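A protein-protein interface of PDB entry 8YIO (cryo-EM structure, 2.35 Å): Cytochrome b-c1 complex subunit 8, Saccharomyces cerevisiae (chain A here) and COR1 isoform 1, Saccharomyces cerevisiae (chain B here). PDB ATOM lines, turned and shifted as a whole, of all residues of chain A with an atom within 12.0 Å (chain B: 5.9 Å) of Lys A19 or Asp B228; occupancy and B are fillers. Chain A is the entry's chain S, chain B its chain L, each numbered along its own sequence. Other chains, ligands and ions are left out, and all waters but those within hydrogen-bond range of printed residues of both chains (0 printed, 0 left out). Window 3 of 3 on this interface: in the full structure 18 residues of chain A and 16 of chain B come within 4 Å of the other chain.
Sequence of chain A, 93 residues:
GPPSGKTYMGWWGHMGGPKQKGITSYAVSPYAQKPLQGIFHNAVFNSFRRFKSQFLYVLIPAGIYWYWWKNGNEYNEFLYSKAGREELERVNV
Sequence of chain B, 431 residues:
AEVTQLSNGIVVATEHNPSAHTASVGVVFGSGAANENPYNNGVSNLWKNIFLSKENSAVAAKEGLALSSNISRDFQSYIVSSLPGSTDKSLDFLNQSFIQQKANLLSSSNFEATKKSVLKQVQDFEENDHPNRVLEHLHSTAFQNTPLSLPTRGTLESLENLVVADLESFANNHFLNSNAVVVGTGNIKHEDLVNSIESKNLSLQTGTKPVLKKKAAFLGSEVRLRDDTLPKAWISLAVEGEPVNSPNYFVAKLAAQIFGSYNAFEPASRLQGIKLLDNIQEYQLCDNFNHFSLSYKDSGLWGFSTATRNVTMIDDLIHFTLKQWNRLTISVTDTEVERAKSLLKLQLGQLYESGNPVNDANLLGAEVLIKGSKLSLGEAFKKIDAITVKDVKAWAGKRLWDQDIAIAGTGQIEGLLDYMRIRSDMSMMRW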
ATOM      1  N   TRP A  11      25.075  -5.023 -19.238  1.00  0.00           N
ATOM      2  CA  TRP A  11      25.349  -3.792 -18.510  1.00  0.00           C
ATOM      3  C   TRP A  11      24.262  -3.611 -17.456  1.00  0.00           C
ATOM      4  O   TRP A  11      23.415  -4.486 -17.269  1.00  0.00           O
ATOM      5  CB  TRP A  11      25.438  -2.594 -19.467  1.00  0.00           C
ATOM      6  CG  TRP A  11      26.382  -1.510 -19.016  1.00  0.00           C
ATOM      7  CD1 TRP A  11      26.045  -0.258 -18.594  1.00  0.00           C
ATOM      8  CD2 TRP A  11      27.811  -1.584 -18.943  1.00  0.00           C
ATOM      9  NE1 TRP A  11      27.170   0.450 -18.263  1.00  0.00           N
ATOM     10  CE2 TRP A  11      28.269  -0.340 -18.469  1.00  0.00           C
ATOM     11  CE3 TRP A  11      28.748  -2.582 -19.230  1.00  0.00           C
ATOM     12  CZ2 TRP A  11      29.623  -0.064 -18.278  1.00  0.00           C
ATOM     13  CZ3 TRP A  11      30.090  -2.308 -19.038  1.00  0.00           C
ATOM     14  CH2 TRP A  11      30.514  -1.058 -18.568  1.00  0.00           C
ATOM     15  N   TRP A  12      24.296  -2.470 -16.759  1.00  0.00           N
ATOM     16  CA  TRP A  12      23.379  -2.206 -15.648  1.00  0.00           C
ATOM     17  C   TRP A  12      21.936  -2.110 -16.137  1.00  0.00           C
ATOM     18  O   TRP A  12      21.605  -1.261 -16.970  1.00  0.00           O
ATOM     19  CB  TRP A  12      23.774  -0.916 -14.929  1.00  0.00           C
ATOM     20  CG  TRP A  12      25.150  -0.915 -14.317  1.00  0.00           C
ATOM     21  CD1 TRP A  12      26.255  -0.279 -14.797  1.00  0.00           C
ATOM     22  CD2 TRP A  12      25.557  -1.562 -13.105  1.00  0.00           C
ATOM     23  NE1 TRP A  12      27.325  -0.497 -13.969  1.00  0.00           N
ATOM     24  CE2 TRP A  12      26.923  -1.281 -12.921  1.00  0.00           C
ATOM     25  CE3 TRP A  12      24.900  -2.357 -12.160  1.00  0.00           C
ATOM     26  CZ2 TRP A  12      27.647  -1.765 -11.832  1.00  0.00           C
ATOM     27  CZ3 TRP A  12      25.617  -2.836 -11.082  1.00  0.00           C
ATOM     28  CH2 TRP A  12      26.977  -2.539 -10.926  1.00  0.00           C
ATOM     29  N   GLY A  13      21.078  -2.990 -15.617  1.00  0.00           N
ATOM     30  CA  GLY A  13      19.705  -3.114 -16.042  1.00  0.00           C
ATOM     31  C   GLY A  13      19.433  -4.312 -16.935  1.00  0.00           C
ATOM     32  O   GLY A  13      18.305  -4.814 -16.951  1.00  0.00           O
ATOM     33  N   HIS A  14      20.430  -4.763 -17.693  1.00  0.00           N
ATOM     34  CA  HIS A  14      20.305  -5.919 -18.580  1.00  0.00           C
ATOM     35  C   HIS A  14      21.551  -6.803 -18.474  1.00  0.00           C
ATOM     36  O   HIS A  14      22.182  -7.148 -19.473  1.00  0.00           O
ATOM     37  CB  HIS A  14      20.035  -5.484 -20.023  1.00  0.00           C
ATOM     38  CG  HIS A  14      21.022  -4.493 -20.566  1.00  0.00           C
ATOM     39  ND1 HIS A  14      21.008  -3.158 -20.219  1.00  0.00           N
ATOM     40  CD2 HIS A  14      22.042  -4.643 -21.441  1.00  0.00           C
ATOM     41  CE1 HIS A  14      21.984  -2.531 -20.851  1.00  0.00           C
ATOM     42  NE2 HIS A  14      22.626  -3.410 -21.599  1.00  0.00           N
ATOM     43  N   MET A  15      21.924  -7.159 -17.239  1.00  0.00           N
ATOM     44  CA  MET A  15      23.208  -7.812 -16.977  1.00  0.00           C
ATOM     45  C   MET A  15      23.284  -9.227 -17.546  1.00  0.00           C
ATOM     46  O   MET A  15      24.369  -9.677 -17.927  1.00  0.00           O
ATOM     47  CB  MET A  15      23.482  -7.831 -15.473  1.00  0.00           C
ATOM     48  CG  MET A  15      24.941  -8.058 -15.093  1.00  0.00           C
ATOM     49  SD  MET A  15      26.039  -6.713 -15.593  1.00  0.00           S
ATOM     50  CE  MET A  15      25.449  -5.380 -14.558  1.00  0.00           C
ATOM     51  N   GLY A  16      22.169  -9.936 -17.616  1.00  0.00           N
ATOM     52  CA  GLY A  16      22.118 -11.218 -18.275  1.00  0.00           C
ATOM     53  C   GLY A  16      22.119 -12.456 -17.394  1.00  0.00           C
ATOM     54  O   GLY A  16      22.556 -13.514 -17.857  1.00  0.00           O
ATOM     55  N   GLY A  17      21.652 -12.360 -16.154  1.00  0.00           N
ATOM     56  CA  GLY A  17      21.501 -13.519 -15.309  1.00  0.00           C
ATOM     57  C   GLY A  17      20.076 -14.034 -15.328  1.00  0.00           C
ATOM     58  O   GLY A  17      19.255 -13.612 -16.149  1.00  0.00           O
ATOM     59  N   PRO A  18      19.752 -14.958 -14.430  1.00  0.00           N
ATOM     60  CA  PRO A  18      18.365 -15.425 -14.320  1.00  0.00           C
ATOM     61  C   PRO A  18      17.488 -14.388 -13.631  1.00  0.00           C
ATOM     62  O   PRO A  18      17.957 -13.406 -13.055  1.00  0.00           O
ATOM     63  CB  PRO A  18      18.488 -16.701 -13.486  1.00  0.00           C
ATOM     64  CG  PRO A  18      19.706 -16.489 -12.664  1.00  0.00           C
ATOM     65  CD  PRO A  18      20.650 -15.677 -13.512  1.00  0.00           C
ATOM     66  N   LYS A  19      16.181 -14.624 -13.703  1.00  0.00           N
ATOM     67  CA  LYS A  19      15.220 -13.740 -13.062  1.00  0.00           C
ATOM     68  C   LYS A  19      15.167 -14.006 -11.565  1.00  0.00           C
ATOM     69  O   LYS A  19      15.131 -15.156 -11.123  1.00  0.00           O
ATOM     70  CB  LYS A  19      13.835 -13.921 -13.680  1.00  0.00           C
ATOM     71  CG  LYS A  19      13.700 -13.290 -15.046  1.00  0.00           C
ATOM     72  CD  LYS A  19      12.253 -13.189 -15.472  1.00  0.00           C
ATOM     73  CE  LYS A  19      12.124 -12.431 -16.777  1.00  0.00           C
ATOM     74  NZ  LYS A  19      10.788 -11.802 -16.921  1.00  0.00           N
ATOM     75  N   GLN A  20      15.170 -12.933 -10.784  1.00  0.00           N
ATOM     76  CA  GLN A  20      15.195 -13.014  -9.333  1.00  0.00           C
ATOM     77  C   GLN A  20      13.833 -12.649  -8.762  1.00  0.00           C
ATOM     78  O   GLN A  20      13.201 -11.686  -9.203  1.00  0.00           O
ATOM     79  CB  GLN A  20      16.265 -12.087  -8.752  1.00  0.00           C
ATOM     80  CG  GLN A  20      17.665 -12.374  -9.244  1.00  0.00           C
ATOM     81  CD  GLN A  20      18.707 -11.529  -8.547  1.00  0.00           C
ATOM     82  OE1 GLN A  20      18.500 -11.074  -7.425  1.00  0.00           O
ATOM     83  NE2 GLN A  20      19.835 -11.314  -9.211  1.00  0.00           N
ATOM     84  N   LYS A  21      13.395 -13.418  -7.769  1.00  0.00           N
ATOM     85  CA  LYS A  21      12.117 -13.186  -7.111  1.00  0.00           C
ATOM     86  C   LYS A  21      12.163 -13.808  -5.725  1.00  0.00           C
ATOM     87  O   LYS A  21      12.484 -14.989  -5.590  1.00  0.00           O
ATOM     88  CB  LYS A  21      10.967 -13.777  -7.932  1.00  0.00           C
ATOM     89  CG  LYS A  21       9.582 -13.323  -7.521  1.00  0.00           C
ATOM     90  CD  LYS A  21       8.546 -13.854  -8.489  1.00  0.00           C
ATOM     91  CE  LYS A  21       7.164 -13.930  -7.865  1.00  0.00           C
ATOM     92  NZ  LYS A  21       6.520 -12.605  -7.718  1.00  0.00           N
ATOM     93  N   GLY A  22      11.860 -13.012  -4.703  1.00  0.00           N
ATOM     94  CA  GLY A  22      11.740 -13.513  -3.351  1.00  0.00           C
ATOM     95  C   GLY A  22      12.901 -13.227  -2.423  1.00  0.00           C
ATOM     96  O   GLY A  22      12.875 -13.691  -1.280  1.00  0.00           O
ATOM     97  N   ILE A  23      13.904 -12.474  -2.862  1.00  0.00           N
ATOM     98  CA  ILE A  23      15.105 -12.205  -2.077  1.00  0.00           C
ATOM     99  C   ILE A  23      15.080 -10.752  -1.620  1.00  0.00           C
ATOM    100  O   ILE A  23      14.919  -9.840  -2.438  1.00  0.00           O
ATOM    101  CB  ILE A  23      16.378 -12.508  -2.888  1.00  0.00           C
ATOM    102  CG1 ILE A  23      16.361 -13.955  -3.382  1.00  0.00           C
ATOM    103  CG2 ILE A  23      17.624 -12.232  -2.067  1.00  0.00           C
ATOM    104  CD1 ILE A  23      17.523 -14.320  -4.259  1.00  0.00           C
ATOM    105  N   THR A  24      15.237 -10.540  -0.315  1.00  0.00           N
ATOM    106  CA  THR A  24      15.317  -9.216   0.285  1.00  0.00           C
ATOM    107  C   THR A  24      16.710  -9.002   0.867  1.00  0.00           C
ATOM    108  O   THR A  24      17.299  -9.926   1.433  1.00  0.00           O
ATOM    109  CB  THR A  24      14.252  -9.052   1.379  1.00  0.00           C
ATOM    110  OG1 THR A  24      13.010  -9.587   0.914  1.00  0.00           O
ATOM    111  CG2 THR A  24      14.042  -7.593   1.739  1.00  0.00           C
ATOM    112  N   ARG B 226      13.752  -7.044  -4.758  1.00  0.00           N
ATOM    113  CA  ARG B 226      13.857  -7.161  -6.207  1.00  0.00           C
ATOM    114  C   ARG B 226      12.853  -8.175  -6.751  1.00  0.00           C
ATOM    115  O   ARG B 226      12.742  -9.292  -6.238  1.00  0.00           O
ATOM    116  CB  ARG B 226      15.279  -7.551  -6.598  1.00  0.00           C
ATOM    117  CG  ARG B 226      15.505  -7.661  -8.086  1.00  0.00           C
ATOM    118  CD  ARG B 226      16.977  -7.687  -8.423  1.00  0.00           C
ATOM    119  NE  ARG B 226      17.211  -8.254  -9.744  1.00  0.00           N
ATOM    120  CZ  ARG B 226      18.401  -8.331 -10.327  1.00  0.00           C
ATOM    121  NH1 ARG B 226      18.514  -8.866 -11.531  1.00  0.00           N
ATOM    122  NH2 ARG B 226      19.475  -7.874  -9.706  1.00  0.00           N
ATOM    123  N   ASP B 227      12.120  -7.778  -7.795  1.00  0.00           N
ATOM    124  CA  ASP B 227      11.095  -8.615  -8.423  1.00  0.00           C
ATOM    125  C   ASP B 227      11.145  -8.362  -9.929  1.00  0.00           C
ATOM    126  O   ASP B 227      10.599  -7.371 -10.417  1.00  0.00           O
ATOM    127  CB  ASP B 227       9.716  -8.313  -7.850  1.00  0.00           C
ATOM    128  CG  ASP B 227       8.717  -9.436  -8.081  1.00  0.00           C
ATOM    129  OD1 ASP B 227       8.894 -10.228  -9.026  1.00  0.00           O
ATOM    130  OD2 ASP B 227       7.741  -9.526  -7.312  1.00  0.00           O
ATOM    131  N   ASP B 228      11.768  -9.283 -10.662  1.00  0.00           N
ATOM    132  CA  ASP B 228      12.004  -9.106 -12.089  1.00  0.00           C
ATOM    133  C   ASP B 228      10.780  -9.386 -12.953  1.00  0.00           C
ATOM    134  O   ASP B 228      10.822  -9.105 -14.154  1.00  0.00           O
ATOM    135  CB  ASP B 228      13.159 -10.000 -12.540  1.00  0.00           C
ATOM    136  CG  ASP B 228      14.508  -9.442 -12.157  1.00  0.00           C
ATOM    137  OD1 ASP B 228      14.597  -8.223 -11.913  1.00  0.00           O
ATOM    138  OD2 ASP B 228      15.481 -10.218 -12.099  1.00  0.00           O
ATOM    139  N   THR B 229       9.702  -9.920 -12.388  1.00  0.00           N
ATOM    140  CA  THR B 229       8.487 -10.190 -13.145  1.00  0.00           C
ATOM    141  C   THR B 229       7.504  -9.022 -13.144  1.00  0.00           C
ATOM    142  O   THR B 229       6.442  -9.132 -13.762  1.00  0.00           O
ATOM    143  CB  THR B 229       7.791 -11.449 -12.609  1.00  0.00           C
ATOM    144  OG1 THR B 229       7.302 -11.209 -11.285  1.00  0.00           O
ATOM    145  CG2 THR B 229       8.757 -12.620 -12.577  1.00  0.00           C
ATOM    146  N   LEU B 230       7.827  -7.907 -12.466  1.00  0.00           N
ATOM    147  CA  LEU B 230       7.042  -6.680 -12.455  1.00  0.00           C
ATOM    148  C   LEU B 230       7.502  -5.748 -13.575  1.00  0.00           C
ATOM    149  O   LEU B 230       8.681  -5.745 -13.939  1.00  0.00           O
ATOM    150  CB  LEU B 230       7.171  -5.979 -11.100  1.00  0.00           C
ATOM    151  CG  LEU B 230       6.655  -6.744  -9.877  1.00  0.00           C
ATOM    152  CD1 LEU B 230       6.813  -5.927  -8.608  1.00  0.00           C
ATOM    153  CD2 LEU B 230       5.209  -7.169 -10.056  1.00  0.00           C
ATOM    154  N   GLY B 411      10.738  -4.081  -7.596  1.00  0.00           N
ATOM    155  CA  GLY B 411      10.619  -4.257  -9.029  1.00  0.00           C
ATOM    156  C   GLY B 411      11.942  -4.491  -9.727  1.00  0.00           C
ATOM    157  O   GLY B 411      12.811  -5.187  -9.200  1.00  0.00           O
ATOM    158  N   GLN B 412      12.113  -3.907 -10.912  1.00  0.00           N
ATOM    159  CA  GLN B 412      13.331  -4.088 -11.703  1.00  0.00           C
ATOM    160  C   GLN B 412      14.353  -3.031 -11.295  1.00  0.00           C
ATOM    161  O   GLN B 412      14.548  -2.014 -11.958  1.00  0.00           O
ATOM    162  CB  GLN B 412      13.013  -4.025 -13.190  1.00  0.00           C
ATOM    163  CG  GLN B 412      12.123  -5.154 -13.681  1.00  0.00           C
ATOM    164  CD  GLN B 412      11.967  -5.164 -15.188  1.00  0.00           C
ATOM    165  OE1 GLN B 412      12.947  -5.098 -15.924  1.00  0.00           O
ATOM    166  NE2 GLN B 412      10.730  -5.245 -15.653  1.00  0.00           N
ATOM    167  N   ILE B 413      15.038  -3.300 -10.186  1.00  0.00           N
ATOM    168  CA  ILE B 413      15.907  -2.317  -9.550  1.00  0.00           C
ATOM    169  C   ILE B 413      17.368  -2.740  -9.637  1.00  0.00           C
ATOM    170  O   ILE B 413      18.168  -2.409  -8.758  1.00  0.00           O
ATOM    171  CB  ILE B 413      15.496  -2.089  -8.083  1.00  0.00           C
ATOM    172  CG1 ILE B 413      15.299  -3.430  -7.370  1.00  0.00           C
ATOM    173  CG2 ILE B 413      14.242  -1.246  -8.013  1.00  0.00           C
ATOM    174  CD1 ILE B 413      15.232  -3.327  -5.870  1.00  0.00           C
ATOM    175  N   GLU B 414      17.721  -3.473 -10.693  1.00  0.00           N
ATOM    176  CA  GLU B 414      19.104  -3.904 -10.882  1.00  0.00           C
ATOM    177  C   GLU B 414      20.022  -2.725 -11.186  1.00  0.00           C
ATOM    178  O   GLU B 414      21.177  -2.703 -10.752  1.00  0.00           O
ATOM    179  CB  GLU B 414      19.176  -4.937 -12.005  1.00  0.00           C
ATOM    180  CG  GLU B 414      20.512  -5.637 -12.123  1.00  0.00           C
ATOM    181  CD  GLU B 414      20.825  -6.062 -13.540  1.00  0.00           C
ATOM    182  OE1 GLU B 414      21.482  -5.287 -14.262  1.00  0.00           O
ATOM    183  OE2 GLU B 414      20.415  -7.170 -13.934  1.00  0.00           O
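Of the 9 printed residues of chain B, 5 touch a printed residue of chain A.
Hydrophobic or aromatic side chains of chain A that line the printed part of chain B: Trp A12 and Met A15.
The side-chain amide nitrogen (NE2) of Gln A20 sits close to the guanidinium group (NH2) of Arg B226 (3.5 Å).
OD2 of Asp B227 lies within salt-bridge range of NZ of Lys A21 (3.3 Å).
The side-chain carboxylate (OD2) of Asp B228 is in hydrogen-bond range of the backbone NH (N) of Gln A20.
The side-chain carboxylate of Glu B414 lies within hydrogen-bond range of the backbone NH of Gly A13 (2.7 Å).
The side-chain carboxylate (OD2) of Asp B228 lies within salt-bridge range of the guanidinium group (NH1) of Arg B226 (3.4 Å).
The guanidinium group of Arg B226 lies within salt-bridge range of the side-chain carboxylate of Glu B414 (3.5 Å).
OD1 of Asp B227 lies within hydrogen-bond range of OG1 of Thr B229, at 2.9 Å.
N of Asp B227 lies within hydrogen-bond range of O of Gly B411 (3.0 Å).
Printed residues of chain B within 4 Å of Trp A11: Glu B414.
Of the printed residues of chain B, His A14 touches Glu B414 (3.6 Å).
Printed residues of chain B within 4 Å of Lys A19: Asp B228.
Of the printed residues of chain B, Ile A23 touches Arg B226.
Of the printed residues of chain A, Arg B226 touches Gln A20 and Ile A23.
Asp B227 touches two residues of chain A.
Asp B228 touches just these residues of chain A: Lys A19 (3.7 Å) and Gln A20 (3.0 Å).
Of chain A, only Lys A21 (3.9 Å) comes within 4 Å of Thr B229.
No residue of chain A comes within 4 Å of Leu B230.
No residue of chain A comes within 4 Å of Gly B411.
No residue of chain A comes within 4 Å of Gln B412.
Of the printed residues of chain A, Glu B414 touches Trp A11 (3.7 Å), Trp A12 (3.7 Å), Gly A13 (2.7 Å), His A14 (3.6 Å) and Met A15 (3.5 Å).
Among the printed residues, pairs that only touch across the chains: Trp A11 with Glu B414 (3.7 Å), Trp A12 with Glu B414 (3.7 Å), His A14 with Glu B414 (3.6 Å), Met A15 with Glu B414 (3.5 Å), Lys A19 with Asp B228 (3.7 Å), Gln A20 with Asp B227 (3.8 Å), Lys A21 with Thr B229 (3.9 Å) and Ile A23 with Arg B226 (3.8 Å).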
